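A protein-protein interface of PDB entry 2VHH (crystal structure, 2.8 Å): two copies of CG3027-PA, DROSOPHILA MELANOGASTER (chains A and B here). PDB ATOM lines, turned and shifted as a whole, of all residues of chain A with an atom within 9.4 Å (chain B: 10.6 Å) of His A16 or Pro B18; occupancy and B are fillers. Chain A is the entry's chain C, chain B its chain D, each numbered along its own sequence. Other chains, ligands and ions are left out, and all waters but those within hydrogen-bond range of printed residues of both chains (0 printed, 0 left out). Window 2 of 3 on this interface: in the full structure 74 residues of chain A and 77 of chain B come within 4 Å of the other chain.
Of the 17 printed residues of chain B, 8 touch a printed residue of chain A.
Hydrophobic or aromatic side chains of chain B within 4 Å of the printed part of chain A: His B16, Leu B17, Pro B18 and Val B25.
Along chain B the printed residues that touch a printed residue of chain A span positions 12 to 25.
Of the 18 printed residues of chain A, 8 touch a printed residue of chain B.
Among the printed residues, no Asp or Glu carboxylate lies within 4 Å of a Lys or Arg side-chain nitrogen of the other chain.
The side-chain sulfur (SG) of Cys A12 sits at hydrogen-bond distance from the side-chain carboxylate (OE1) of Glu B21 (3.3 Å).
OE1 of Glu A5 lies close to O of Asp B20 (3.4 Å).
Of the printed residues of chain B, Leu A6 touches Glu B24.
Cys A12 touches one residue of chain B.
Of chain B, only His B16 (3.4 Å), Leu B17 (3.4 Å), Pro B18 (3.8 Å) and Glu B21 (3.3 Å) come within 4 Å of His A16.
No residue of chain B comes within 4 Å of Leu A17.
Printed residues of chain B within 4 Å of Pro A18: His B16.
Pro A19 touches none of the printed residues of chain B.
Of the printed residues of chain A, His B16 touches His A16 (3.4 Å), Pro A18 (3.4 Å) and Glu A21 (3.2 Å).
Pro B18 touches just one residue of chain A: His A16 (3.8 Å).
No residue of chain A comes within 4 Å of Pro B19.
Of chain A, only Glu A5 comes within 4 Å of Asp B20.
Of chain A, only Cys A12 and His A16 come within 4 Å of Glu B21.
Of the printed residues of chain A, Glu B24 touches Glu A5 and Leu A6.
The nearest residue of chain B that does not touch His A16 is Lys B15 (6.4 Å).
Cys A12 touches Glu B21, but with the chains exchanged Glu A21 does not touch Cys B12 (4.5 Å).
His A16 touches Leu B17, but with the chains exchanged Leu A17 does not touch His B16 (4.2 Å).
His A16 touches Pro B18, and with the chains exchanged Pro A18 touches His B16.
His A16 touches Glu B21, and with the chains exchanged Glu A21 touches His B16.
12 positions are printed for both chains.
Of the 12 pairs that touch across the chains among the printed residues, 5 have their exchanged pair printed and touching as well.
A ring nitrogen (ND1) of His A16 is in hydrogen-bond range of the backbone carbonyl oxygen (O) of Cys A12, at 2.9 Å.
O of Cys B12 is in hydrogen-bond range of ND1 of His B16, 2.9 Å away.
Among the printed residues, merely in contact across the chains: Glu A21 with His B16 (3.2 Å), His A16 with Glu B21 (3.3 Å), Pro A18 with His B16 (3.4 Å), His A16 with His B16 (3.4 Å), His A16 with Leu B17 (3.4 Å), Leu A6 with Glu B24 (3.7 Å), Glu A5 with Glu B24 (3.7 Å), His A16 with Pro B18 (3.8 Å), Leu A9 with Val B25 (3.9 Å) and Val A25 with Cys B12 (3.95 Å).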
ATOM      1  N   GLU A   5       6.267 -26.037  21.283  1.00  0.00           N
ATOM      2  CA  GLU A   5       6.060 -24.669  20.717  1.00  0.00           C
ATOM      3  C   GLU A   5       5.289 -23.722  21.662  1.00  0.00           C
ATOM      4  O   GLU A   5       5.441 -22.499  21.585  1.00  0.00           O
ATOM      5  CB  GLU A   5       5.424 -24.748  19.316  1.00  0.00           C
ATOM      6  CG  GLU A   5       4.051 -25.427  19.230  1.00  0.00           C
ATOM      7  CD  GLU A   5       2.914 -24.450  18.920  1.00  0.00           C
ATOM      8  OE1 GLU A   5       1.752 -24.897  18.836  1.00  0.00           O
ATOM      9  OE2 GLU A   5       3.168 -23.237  18.751  1.00  0.00           O
ATOM     10  N   LEU A   6       4.487 -24.292  22.561  1.00  0.00           N
ATOM     11  CA  LEU A   6       3.715 -23.519  23.540  1.00  0.00           C
ATOM     12  C   LEU A   6       4.593 -23.042  24.706  1.00  0.00           C
ATOM     13  O   LEU A   6       5.382 -23.818  25.251  1.00  0.00           O
ATOM     14  CB  LEU A   6       2.550 -24.364  24.066  1.00  0.00           C
ATOM     15  CG  LEU A   6       1.330 -23.623  24.615  1.00  0.00           C
ATOM     16  CD1 LEU A   6       0.431 -23.151  23.478  1.00  0.00           C
ATOM     17  CD2 LEU A   6       0.557 -24.515  25.578  1.00  0.00           C
ATOM     18  N   LYS A   7       4.449 -21.770  25.088  1.00  0.00           N
ATOM     19  CA  LYS A   7       5.267 -21.185  26.163  1.00  0.00           C
ATOM     20  C   LYS A   7       4.510 -20.997  27.487  1.00  0.00           C
ATOM     21  O   LYS A   7       5.108 -21.113  28.557  1.00  0.00           O
ATOM     22  CB  LYS A   7       5.923 -19.856  25.737  1.00  0.00           C
ATOM     23  CG  LYS A   7       6.826 -19.908  24.488  1.00  0.00           C
ATOM     24  CD  LYS A   7       6.204 -19.137  23.308  1.00  0.00           C
ATOM     25  CE  LYS A   7       5.032 -19.898  22.654  1.00  0.00           C
ATOM     26  NZ  LYS A   7       3.894 -19.034  22.199  1.00  0.00           N
ATOM     27  N   ASN A   8       3.209 -20.710  27.413  1.00  0.00           N
ATOM     28  CA  ASN A   8       2.388 -20.474  28.609  1.00  0.00           C
ATOM     29  C   ASN A   8       0.879 -20.582  28.317  1.00  0.00           C
ATOM     30  O   ASN A   8       0.351 -19.804  27.519  1.00  0.00           O
ATOM     31  CB  ASN A   8       2.739 -19.101  29.200  1.00  0.00           C
ATOM     32  CG  ASN A   8       2.173 -18.883  30.598  1.00  0.00           C
ATOM     33  OD1 ASN A   8       1.418 -19.703  31.140  1.00  0.00           O
ATOM     34  ND2 ASN A   8       2.540 -17.753  31.189  1.00  0.00           N
ATOM     35  N   LEU A   9       0.190 -21.533  28.961  1.00  0.00           N
ATOM     36  CA  LEU A   9      -1.218 -21.833  28.626  1.00  0.00           C
ATOM     37  C   LEU A   9      -2.168 -20.660  28.887  1.00  0.00           C
ATOM     38  O   LEU A   9      -3.013 -20.339  28.051  1.00  0.00           O
ATOM     39  CB  LEU A   9      -1.715 -23.102  29.342  1.00  0.00           C
ATOM     40  CG  LEU A   9      -3.220 -23.421  29.280  1.00  0.00           C
ATOM     41  CD1 LEU A   9      -3.622 -24.011  27.943  1.00  0.00           C
ATOM     42  CD2 LEU A   9      -3.636 -24.357  30.397  1.00  0.00           C
ATOM     43  N   ASN A  10      -2.021 -20.032  30.047  1.00  0.00           N
ATOM     44  CA  ASN A  10      -2.846 -18.890  30.429  1.00  0.00           C
ATOM     45  C   ASN A  10      -2.720 -17.727  29.433  1.00  0.00           C
ATOM     46  O   ASN A  10      -3.729 -17.132  29.032  1.00  0.00           O
ATOM     47  CB  ASN A  10      -2.487 -18.443  31.855  1.00  0.00           C
ATOM     48  CG  ASN A  10      -3.409 -17.360  32.384  1.00  0.00           C
ATOM     49  OD1 ASN A  10      -4.519 -17.175  31.895  1.00  0.00           O
ATOM     50  ND2 ASN A  10      -2.946 -16.636  33.388  1.00  0.00           N
ATOM     51  N   ASP A  11      -1.479 -17.432  29.034  1.00  0.00           N
ATOM     52  CA  ASP A  11      -1.174 -16.389  28.049  1.00  0.00           C
ATOM     53  C   ASP A  11      -1.775 -16.712  26.684  1.00  0.00           C
ATOM     54  O   ASP A  11      -2.176 -15.812  25.938  1.00  0.00           O
ATOM     55  CB  ASP A  11       0.341 -16.219  27.895  1.00  0.00           C
ATOM     56  CG  ASP A  11       1.004 -15.588  29.122  1.00  0.00           C
ATOM     57  OD1 ASP A  11       0.295 -15.004  29.976  1.00  0.00           O
ATOM     58  OD2 ASP A  11       2.251 -15.668  29.224  1.00  0.00           O
ATOM     59  N   CYS A  12      -1.829 -18.003  26.373  1.00  0.00           N
ATOM     60  CA  CYS A  12      -2.371 -18.490  25.120  1.00  0.00           C
ATOM     61  C   CYS A  12      -3.890 -18.328  25.049  1.00  0.00           C
ATOM     62  O   CYS A  12      -4.426 -17.959  24.006  1.00  0.00           O
ATOM     63  CB  CYS A  12      -1.974 -19.951  24.920  1.00  0.00           C
ATOM     64  SG  CYS A  12      -2.527 -20.684  23.374  1.00  0.00           S
ATOM     65  N   LEU A  13      -4.572 -18.596  26.157  1.00  0.00           N
ATOM     66  CA  LEU A  13      -6.025 -18.490  26.212  1.00  0.00           C
ATOM     67  C   LEU A  13      -6.496 -17.038  26.211  1.00  0.00           C
ATOM     68  O   LEU A  13      -7.505 -16.702  25.586  1.00  0.00           O
ATOM     69  CB  LEU A  13      -6.556 -19.202  27.455  1.00  0.00           C
ATOM     70  CG  LEU A  13      -6.087 -20.638  27.677  1.00  0.00           C
ATOM     71  CD1 LEU A  13      -6.404 -21.077  29.101  1.00  0.00           C
ATOM     72  CD2 LEU A  13      -6.687 -21.590  26.643  1.00  0.00           C
ATOM     73  N   GLU A  14      -5.764 -16.175  26.909  1.00  0.00           N
ATOM     74  CA  GLU A  14      -6.150 -14.766  26.993  1.00  0.00           C
ATOM     75  C   GLU A  14      -5.824 -13.982  25.717  1.00  0.00           C
ATOM     76  O   GLU A  14      -6.176 -12.807  25.594  1.00  0.00           O
ATOM     77  CB  GLU A  14      -5.566 -14.095  28.244  1.00  0.00           C
ATOM     78  CG  GLU A  14      -4.074 -13.812  28.195  1.00  0.00           C
ATOM     79  CD  GLU A  14      -3.500 -13.451  29.560  1.00  0.00           C
ATOM     80  OE1 GLU A  14      -4.158 -13.729  30.590  1.00  0.00           O
ATOM     81  OE2 GLU A  14      -2.379 -12.898  29.601  1.00  0.00           O
ATOM     82  N   LYS A  15      -5.174 -14.646  24.766  1.00  0.00           N
ATOM     83  CA  LYS A  15      -4.839 -14.034  23.487  1.00  0.00           C
ATOM     84  C   LYS A  15      -5.786 -14.478  22.361  1.00  0.00           C
ATOM     85  O   LYS A  15      -5.699 -13.972  21.241  1.00  0.00           O
ATOM     86  CB  LYS A  15      -3.380 -14.344  23.134  1.00  0.00           C
ATOM     87  CG  LYS A  15      -2.752 -13.418  22.092  1.00  0.00           C
ATOM     88  CD  LYS A  15      -1.243 -13.625  21.988  1.00  0.00           C
ATOM     89  CE  LYS A  15      -0.527 -13.161  23.259  1.00  0.00           C
ATOM     90  NZ  LYS A  15       0.951 -13.295  23.155  1.00  0.00           N
ATOM     91  N   HIS A  16      -6.691 -15.413  22.652  1.00  0.00           N
ATOM     92  CA  HIS A  16      -7.573 -15.951  21.613  1.00  0.00           C
ATOM     93  C   HIS A  16      -9.043 -16.054  22.029  1.00  0.00           C
ATOM     94  O   HIS A  16      -9.888 -16.487  21.233  1.00  0.00           O
ATOM     95  CB  HIS A  16      -7.054 -17.299  21.111  1.00  0.00           C
ATOM     96  CG  HIS A  16      -5.705 -17.233  20.466  1.00  0.00           C
ATOM     97  ND1 HIS A  16      -4.531 -17.279  21.187  1.00  0.00           N
ATOM     98  CD2 HIS A  16      -5.341 -17.144  19.164  1.00  0.00           C
ATOM     99  CE1 HIS A  16      -3.503 -17.213  20.361  1.00  0.00           C
ATOM    100  NE2 HIS A  16      -3.966 -17.133  19.127  1.00  0.00           N
ATOM    101  N   LEU A  17      -9.348 -15.640  23.256  1.00  0.00           N
ATOM    102  CA  LEU A  17     -10.709 -15.725  23.788  1.00  0.00           C
ATOM    103  C   LEU A  17     -11.279 -14.352  24.145  1.00  0.00           C
ATOM    104  O   LEU A  17     -10.613 -13.580  24.833  1.00  0.00           O
ATOM    105  CB  LEU A  17     -10.724 -16.607  25.042  1.00  0.00           C
ATOM    106  CG  LEU A  17     -11.028 -18.104  24.944  1.00  0.00           C
ATOM    107  CD1 LEU A  17      -9.964 -18.899  24.195  1.00  0.00           C
ATOM    108  CD2 LEU A  17     -11.182 -18.642  26.336  1.00  0.00           C
ATOM    109  N   PRO A  18     -12.492 -14.025  23.649  1.00  0.00           N
ATOM    110  CA  PRO A  18     -13.273 -12.882  24.140  1.00  0.00           C
ATOM    111  C   PRO A  18     -13.419 -12.857  25.670  1.00  0.00           C
ATOM    112  O   PRO A  18     -13.733 -13.892  26.269  1.00  0.00           O
ATOM    113  CB  PRO A  18     -14.642 -13.088  23.480  1.00  0.00           C
ATOM    114  CG  PRO A  18     -14.323 -13.755  22.196  1.00  0.00           C
ATOM    115  CD  PRO A  18     -13.151 -14.671  22.499  1.00  0.00           C
ATOM    116  N   PRO A  19     -13.204 -11.673  26.296  1.00  0.00           N
ATOM    117  CA  PRO A  19     -13.212 -11.483  27.756  1.00  0.00           C
ATOM    118  C   PRO A  19     -14.392 -12.141  28.485  1.00  0.00           C
ATOM    119  O   PRO A  19     -14.277 -12.489  29.659  1.00  0.00           O
ATOM    120  CB  PRO A  19     -13.288  -9.963  27.907  1.00  0.00           C
ATOM    121  CG  PRO A  19     -12.600  -9.450  26.720  1.00  0.00           C
ATOM    122  CD  PRO A  19     -12.942 -10.397  25.599  1.00  0.00           C
ATOM    123  N   GLU A  21     -16.035 -15.064  27.425  1.00  0.00           N
ATOM    124  CA  GLU A  21     -15.831 -16.510  27.354  1.00  0.00           C
ATOM    125  C   GLU A  21     -14.637 -16.902  28.215  1.00  0.00           C
ATOM    126  O   GLU A  21     -14.669 -17.928  28.900  1.00  0.00           O
ATOM    127  CB  GLU A  21     -15.557 -16.938  25.895  1.00  0.00           C
ATOM    128  CG  GLU A  21     -16.679 -16.657  24.865  1.00  0.00           C
ATOM    129  CD  GLU A  21     -17.465 -17.913  24.445  1.00  0.00           C
ATOM    130  OE1 GLU A  21     -18.237 -18.454  25.272  1.00  0.00           O
ATOM    131  OE2 GLU A  21     -17.326 -18.354  23.277  1.00  0.00           O
ATOM    132  N   LEU A  22     -13.585 -16.081  28.154  1.00  0.00           N
ATOM    133  CA  LEU A  22     -12.368 -16.273  28.955  1.00  0.00           C
ATOM    134  C   LEU A  22     -12.692 -16.400  30.434  1.00  0.00           C
ATOM    135  O   LEU A  22     -12.108 -17.231  31.130  1.00  0.00           O
ATOM    136  CB  LEU A  22     -11.366 -15.125  28.764  1.00  0.00           C
ATOM    137  CG  LEU A  22     -10.127 -15.135  29.681  1.00  0.00           C
ATOM    138  CD1 LEU A  22      -9.023 -16.028  29.121  1.00  0.00           C
ATOM    139  CD2 LEU A  22      -9.590 -13.739  29.933  1.00  0.00           C
ATOM    140  N   VAL A  25     -14.109 -19.994  30.817  1.00  0.00           N
ATOM    141  CA  VAL A  25     -13.068 -20.997  30.651  1.00  0.00           C
ATOM    142  C   VAL A  25     -12.144 -21.011  31.860  1.00  0.00           C
ATOM    143  O   VAL A  25     -11.865 -22.071  32.418  1.00  0.00           O
ATOM    144  CB  VAL A  25     -12.271 -20.765  29.331  1.00  0.00           C
ATOM    145  CG1 VAL A  25     -10.920 -21.474  29.342  1.00  0.00           C
ATOM    146  CG2 VAL A  25     -13.098 -21.213  28.129  1.00  0.00           C
ATOM    147  N   ASP B  11     -16.004 -27.609  22.049  1.00  0.00           N
ATOM    148  CA  ASP B  11     -16.542 -26.874  20.899  1.00  0.00           C
ATOM    149  C   ASP B  11     -16.183 -25.390  20.983  1.00  0.00           C
ATOM    150  O   ASP B  11     -16.001 -24.735  19.961  1.00  0.00           O
ATOM    151  CB  ASP B  11     -18.056 -27.097  20.736  1.00  0.00           C
ATOM    152  CG  ASP B  11     -18.412 -28.570  20.459  1.00  0.00           C
ATOM    153  OD1 ASP B  11     -17.532 -29.328  19.980  1.00  0.00           O
ATOM    154  OD2 ASP B  11     -19.571 -28.972  20.725  1.00  0.00           O
ATOM    155  N   CYS B  12     -16.054 -24.890  22.207  1.00  0.00           N
ATOM    156  CA  CYS B  12     -15.652 -23.512  22.483  1.00  0.00           C
ATOM    157  C   CYS B  12     -14.184 -23.239  22.114  1.00  0.00           C
ATOM    158  O   CYS B  12     -13.875 -22.212  21.507  1.00  0.00           O
ATOM    159  CB  CYS B  12     -15.931 -23.193  23.958  1.00  0.00           C
ATOM    160  SG  CYS B  12     -14.967 -21.866  24.708  1.00  0.00           S
ATOM    161  N   LEU B  13     -13.289 -24.157  22.473  1.00  0.00           N
ATOM    162  CA  LEU B  13     -11.874 -24.037  22.124  1.00  0.00           C
ATOM    163  C   LEU B  13     -11.606 -24.240  20.629  1.00  0.00           C
ATOM    164  O   LEU B  13     -10.739 -23.568  20.063  1.00  0.00           O
ATOM    165  CB  LEU B  13     -11.031 -25.035  22.921  1.00  0.00           C
ATOM    166  CG  LEU B  13     -10.872 -24.974  24.442  1.00  0.00           C
ATOM    167  CD1 LEU B  13     -10.051 -26.166  24.897  1.00  0.00           C
ATOM    168  CD2 LEU B  13     -10.225 -23.680  24.902  1.00  0.00           C
ATOM    169  N   GLU B  14     -12.328 -25.165  19.992  1.00  0.00           N
ATOM    170  CA  GLU B  14     -12.126 -25.437  18.560  1.00  0.00           C
ATOM    171  C   GLU B  14     -12.676 -24.313  17.664  1.00  0.00           C
ATOM    172  O   GLU B  14     -12.471 -24.319  16.452  1.00  0.00           O
ATOM    173  CB  GLU B  14     -12.702 -26.808  18.158  1.00  0.00           C
ATOM    174  CG  GLU B  14     -14.221 -26.831  17.936  1.00  0.00           C
ATOM    175  CD  GLU B  14     -14.704 -28.050  17.145  1.00  0.00           C
ATOM    176  OE1 GLU B  14     -14.126 -29.150  17.305  1.00  0.00           O
ATOM    177  OE2 GLU B  14     -15.676 -27.903  16.367  1.00  0.00           O
ATOM    178  N   LYS B  15     -13.361 -23.360  18.287  1.00  0.00           N
ATOM    179  CA  LYS B  15     -14.012 -22.244  17.620  1.00  0.00           C
ATOM    180  C   LYS B  15     -13.189 -20.957  17.776  1.00  0.00           C
ATOM    181  O   LYS B  15     -13.505 -19.928  17.171  1.00  0.00           O
ATOM    182  CB  LYS B  15     -15.398 -22.049  18.264  1.00  0.00           C
ATOM    183  CG  LYS B  15     -16.254 -20.911  17.718  1.00  0.00           C
ATOM    184  CD  LYS B  15     -17.698 -21.034  18.188  1.00  0.00           C
ATOM    185  CE  LYS B  15     -18.600 -20.016  17.480  1.00  0.00           C
ATOM    186  NZ  LYS B  15     -20.055 -20.341  17.576  1.00  0.00           N
ATOM    187  N   HIS B  16     -12.137 -21.014  18.590  1.00  0.00           N
ATOM    188  CA  HIS B  16     -11.344 -19.828  18.940  1.00  0.00           C
ATOM    189  C   HIS B  16      -9.834 -20.008  18.799  1.00  0.00           C
ATOM    190  O   HIS B  16      -9.081 -19.052  18.975  1.00  0.00           O
ATOM    191  CB  HIS B  16     -11.626 -19.413  20.385  1.00  0.00           C
ATOM    192  CG  HIS B  16     -12.926 -18.697  20.570  1.00  0.00           C
ATOM    193  ND1 HIS B  16     -14.089 -19.344  20.931  1.00  0.00           N
ATOM    194  CD2 HIS B  16     -13.244 -17.387  20.461  1.00  0.00           C
ATOM    195  CE1 HIS B  16     -15.069 -18.463  21.029  1.00  0.00           C
ATOM    196  NE2 HIS B  16     -14.583 -17.268  20.746  1.00  0.00           N
ATOM    197  N   LEU B  17      -9.387 -21.224  18.505  1.00  0.00           N
ATOM    198  CA  LEU B  17      -7.957 -21.492  18.429  1.00  0.00           C
ATOM    199  C   LEU B  17      -7.504 -22.027  17.068  1.00  0.00           C
ATOM    200  O   LEU B  17      -8.181 -22.868  16.476  1.00  0.00           O
ATOM    201  CB  LEU B  17      -7.519 -22.422  19.568  1.00  0.00           C
ATOM    202  CG  LEU B  17      -7.445 -21.832  20.985  1.00  0.00           C
ATOM    203  CD1 LEU B  17      -7.062 -22.906  21.986  1.00  0.00           C
ATOM    204  CD2 LEU B  17      -6.451 -20.694  21.065  1.00  0.00           C
ATOM    205  N   PRO B  18      -6.366 -21.513  16.559  1.00  0.00           N
ATOM    206  CA  PRO B  18      -5.748 -22.033  15.338  1.00  0.00           C
ATOM    207  C   PRO B  18      -5.390 -23.513  15.496  1.00  0.00           C
ATOM    208  O   PRO B  18      -4.854 -23.902  16.538  1.00  0.00           O
ATOM    209  CB  PRO B  18      -4.477 -21.182  15.194  1.00  0.00           C
ATOM    210  CG  PRO B  18      -4.247 -20.580  16.554  1.00  0.00           C
ATOM    211  CD  PRO B  18      -5.607 -20.380  17.123  1.00  0.00           C
ATOM    212  N   PRO B  19      -5.700 -24.338  14.478  1.00  0.00           N
ATOM    213  CA  PRO B  19      -5.487 -25.796  14.480  1.00  0.00           C
ATOM    214  C   PRO B  19      -4.146 -26.277  15.067  1.00  0.00           C
ATOM    215  O   PRO B  19      -4.081 -27.392  15.595  1.00  0.00           O
ATOM    216  CB  PRO B  19      -5.609 -26.182  12.995  1.00  0.00           C
ATOM    217  CG  PRO B  19      -5.842 -24.888  12.244  1.00  0.00           C
ATOM    218  CD  PRO B  19      -6.337 -23.890  13.232  1.00  0.00           C
ATOM    219  N   ASP B  20      -3.104 -25.446  14.986  1.00  0.00           N
ATOM    220  CA  ASP B  20      -1.781 -25.813  15.508  1.00  0.00           C
ATOM    221  C   ASP B  20      -1.654 -25.664  17.034  1.00  0.00           C
ATOM    222  O   ASP B  20      -1.028 -26.500  17.699  1.00  0.00           O
ATOM    223  CB  ASP B  20      -0.647 -25.081  14.757  1.00  0.00           C
ATOM    224  CG  ASP B  20      -0.558 -23.588  15.093  1.00  0.00           C
ATOM    225  OD1 ASP B  20      -1.552 -22.982  15.561  1.00  0.00           O
ATOM    226  OD2 ASP B  20       0.530 -23.012  14.868  1.00  0.00           O
ATOM    227  N   GLU B  21      -2.262 -24.612  17.578  1.00  0.00           N
ATOM    228  CA  GLU B  21      -2.282 -24.391  19.022  1.00  0.00           C
ATOM    229  C   GLU B  21      -3.351 -25.233  19.708  1.00  0.00           C
ATOM    230  O   GLU B  21      -3.154 -25.715  20.828  1.00  0.00           O
ATOM    231  CB  GLU B  21      -2.515 -22.924  19.334  1.00  0.00           C
ATOM    232  CG  GLU B  21      -1.328 -22.050  19.030  1.00  0.00           C
ATOM    233  CD  GLU B  21      -1.528 -20.634  19.506  1.00  0.00           C
ATOM    234  OE1 GLU B  21      -2.578 -20.347  20.119  1.00  0.00           O
ATOM    235  OE2 GLU B  21      -0.632 -19.802  19.269  1.00  0.00           O
ATOM    236  N   LEU B  22      -4.485 -25.402  19.031  1.00  0.00           N
ATOM    237  CA  LEU B  22      -5.542 -26.274  19.510  1.00  0.00           C
ATOM    238  C   LEU B  22      -4.998 -27.672  19.775  1.00  0.00           C
ATOM    239  O   LEU B  22      -5.360 -28.294  20.764  1.00  0.00           O
ATOM    240  CB  LEU B  22      -6.704 -26.312  18.515  1.00  0.00           C
ATOM    241  CG  LEU B  22      -7.998 -26.973  18.986  1.00  0.00           C
ATOM    242  CD1 LEU B  22      -8.672 -26.164  20.076  1.00  0.00           C
ATOM    243  CD2 LEU B  22      -8.930 -27.165  17.811  1.00  0.00           C
ATOM    244  N   LYS B  23      -4.113 -28.141  18.901  1.00  0.00           N
ATOM    245  CA  LYS B  23      -3.454 -29.433  19.059  1.00  0.00           C
ATOM    246  C   LYS B  23      -2.648 -29.496  20.359  1.00  0.00           C
ATOM    247  O   LYS B  23      -2.607 -30.528  21.020  1.00  0.00           O
ATOM    248  CB  LYS B  23      -2.570 -29.711  17.843  1.00  0.00           C
ATOM    249  CG  LYS B  23      -2.421 -31.177  17.492  1.00  0.00           C
ATOM    250  CD  LYS B  23      -2.583 -31.409  15.985  1.00  0.00           C
ATOM    251  CE  LYS B  23      -2.422 -32.892  15.626  1.00  0.00           C
ATOM    252  NZ  LYS B  23      -3.141 -33.258  14.369  1.00  0.00           N
ATOM    253  N   GLU B  24      -2.029 -28.383  20.735  1.00  0.00           N
ATOM    254  CA  GLU B  24      -1.201 -28.348  21.940  1.00  0.00           C
ATOM    255  C   GLU B  24      -2.027 -28.180  23.210  1.00  0.00           C
ATOM    256  O   GLU B  24      -1.724 -28.795  24.232  1.00  0.00           O
ATOM    257  CB  GLU B  24      -0.129 -27.260  21.843  1.00  0.00           C
ATOM    258  CG  GLU B  24       1.100 -27.501  22.725  1.00  0.00           C
ATOM    259  CD  GLU B  24       2.103 -28.482  22.118  1.00  0.00           C
ATOM    260  OE1 GLU B  24       3.304 -28.132  22.041  1.00  0.00           O
ATOM    261  OE2 GLU B  24       1.696 -29.596  21.716  1.00  0.00           O
ATOM    262  N   VAL B  25      -3.070 -27.358  23.148  1.00  0.00           N
ATOM    263  CA  VAL B  25      -3.962 -27.183  24.288  1.00  0.00           C
ATOM    264  C   VAL B  25      -4.745 -28.472  24.559  1.00  0.00           C
ATOM    265  O   VAL B  25      -4.797 -28.927  25.701  1.00  0.00           O
ATOM    266  CB  VAL B  25      -4.871 -25.932  24.139  1.00  0.00           C
ATOM    267  CG1 VAL B  25      -5.893 -25.864  25.250  1.00  0.00           C
ATOM    268  CG2 VAL B  25      -4.033 -24.668  24.151  1.00  0.00           C
ATOM    269  N   LYS B  26      -5.311 -29.081  23.517  1.00  0.00           N
ATOM    270  CA  LYS B  26      -6.006 -30.365  23.663  1.00  0.00           C
ATOM    271  C   LYS B  26      -5.128 -31.441  24.299  1.00  0.00           C
ATOM    272  O   LYS B  26      -5.614 -32.237  25.086  1.00  0.00           O
ATOM    273  CB  LYS B  26      -6.533 -30.870  22.322  1.00  0.00           C
ATOM    274  CG  LYS B  26      -7.895 -30.346  21.903  1.00  0.00           C
ATOM    275  CD  LYS B  26      -8.537 -31.362  20.962  1.00  0.00           C
ATOM    276  CE  LYS B  26      -9.318 -30.722  19.822  1.00  0.00           C
ATOM    277  NZ  LYS B  26     -10.709 -30.365  20.207  1.00  0.00           N
ATOM    278  N   GLU B  33      -3.954 -35.118  21.110  1.00  0.00           N
ATOM    279  CA  GLU B  33      -3.866 -33.947  20.225  1.00  0.00           C
ATOM    280  C   GLU B  33      -5.194 -33.650  19.520  1.00  0.00           C
ATOM    281  O   GLU B  33      -5.620 -32.497  19.444  1.00  0.00           O
ATOM    282  CB  GLU B  33      -2.736 -34.130  19.195  1.00  0.00           C
ATOM    283  CG  GLU B  33      -2.669 -35.518  18.528  1.00  0.00           C
ATOM    284  CD  GLU B  33      -2.064 -36.579  19.447  1.00  0.00           C
ATOM    285  OE1 GLU B  33      -0.861 -36.456  19.787  1.00  0.00           O
ATOM    286  OE2 GLU B  33      -2.797 -37.525  19.838  1.00  0.00           O
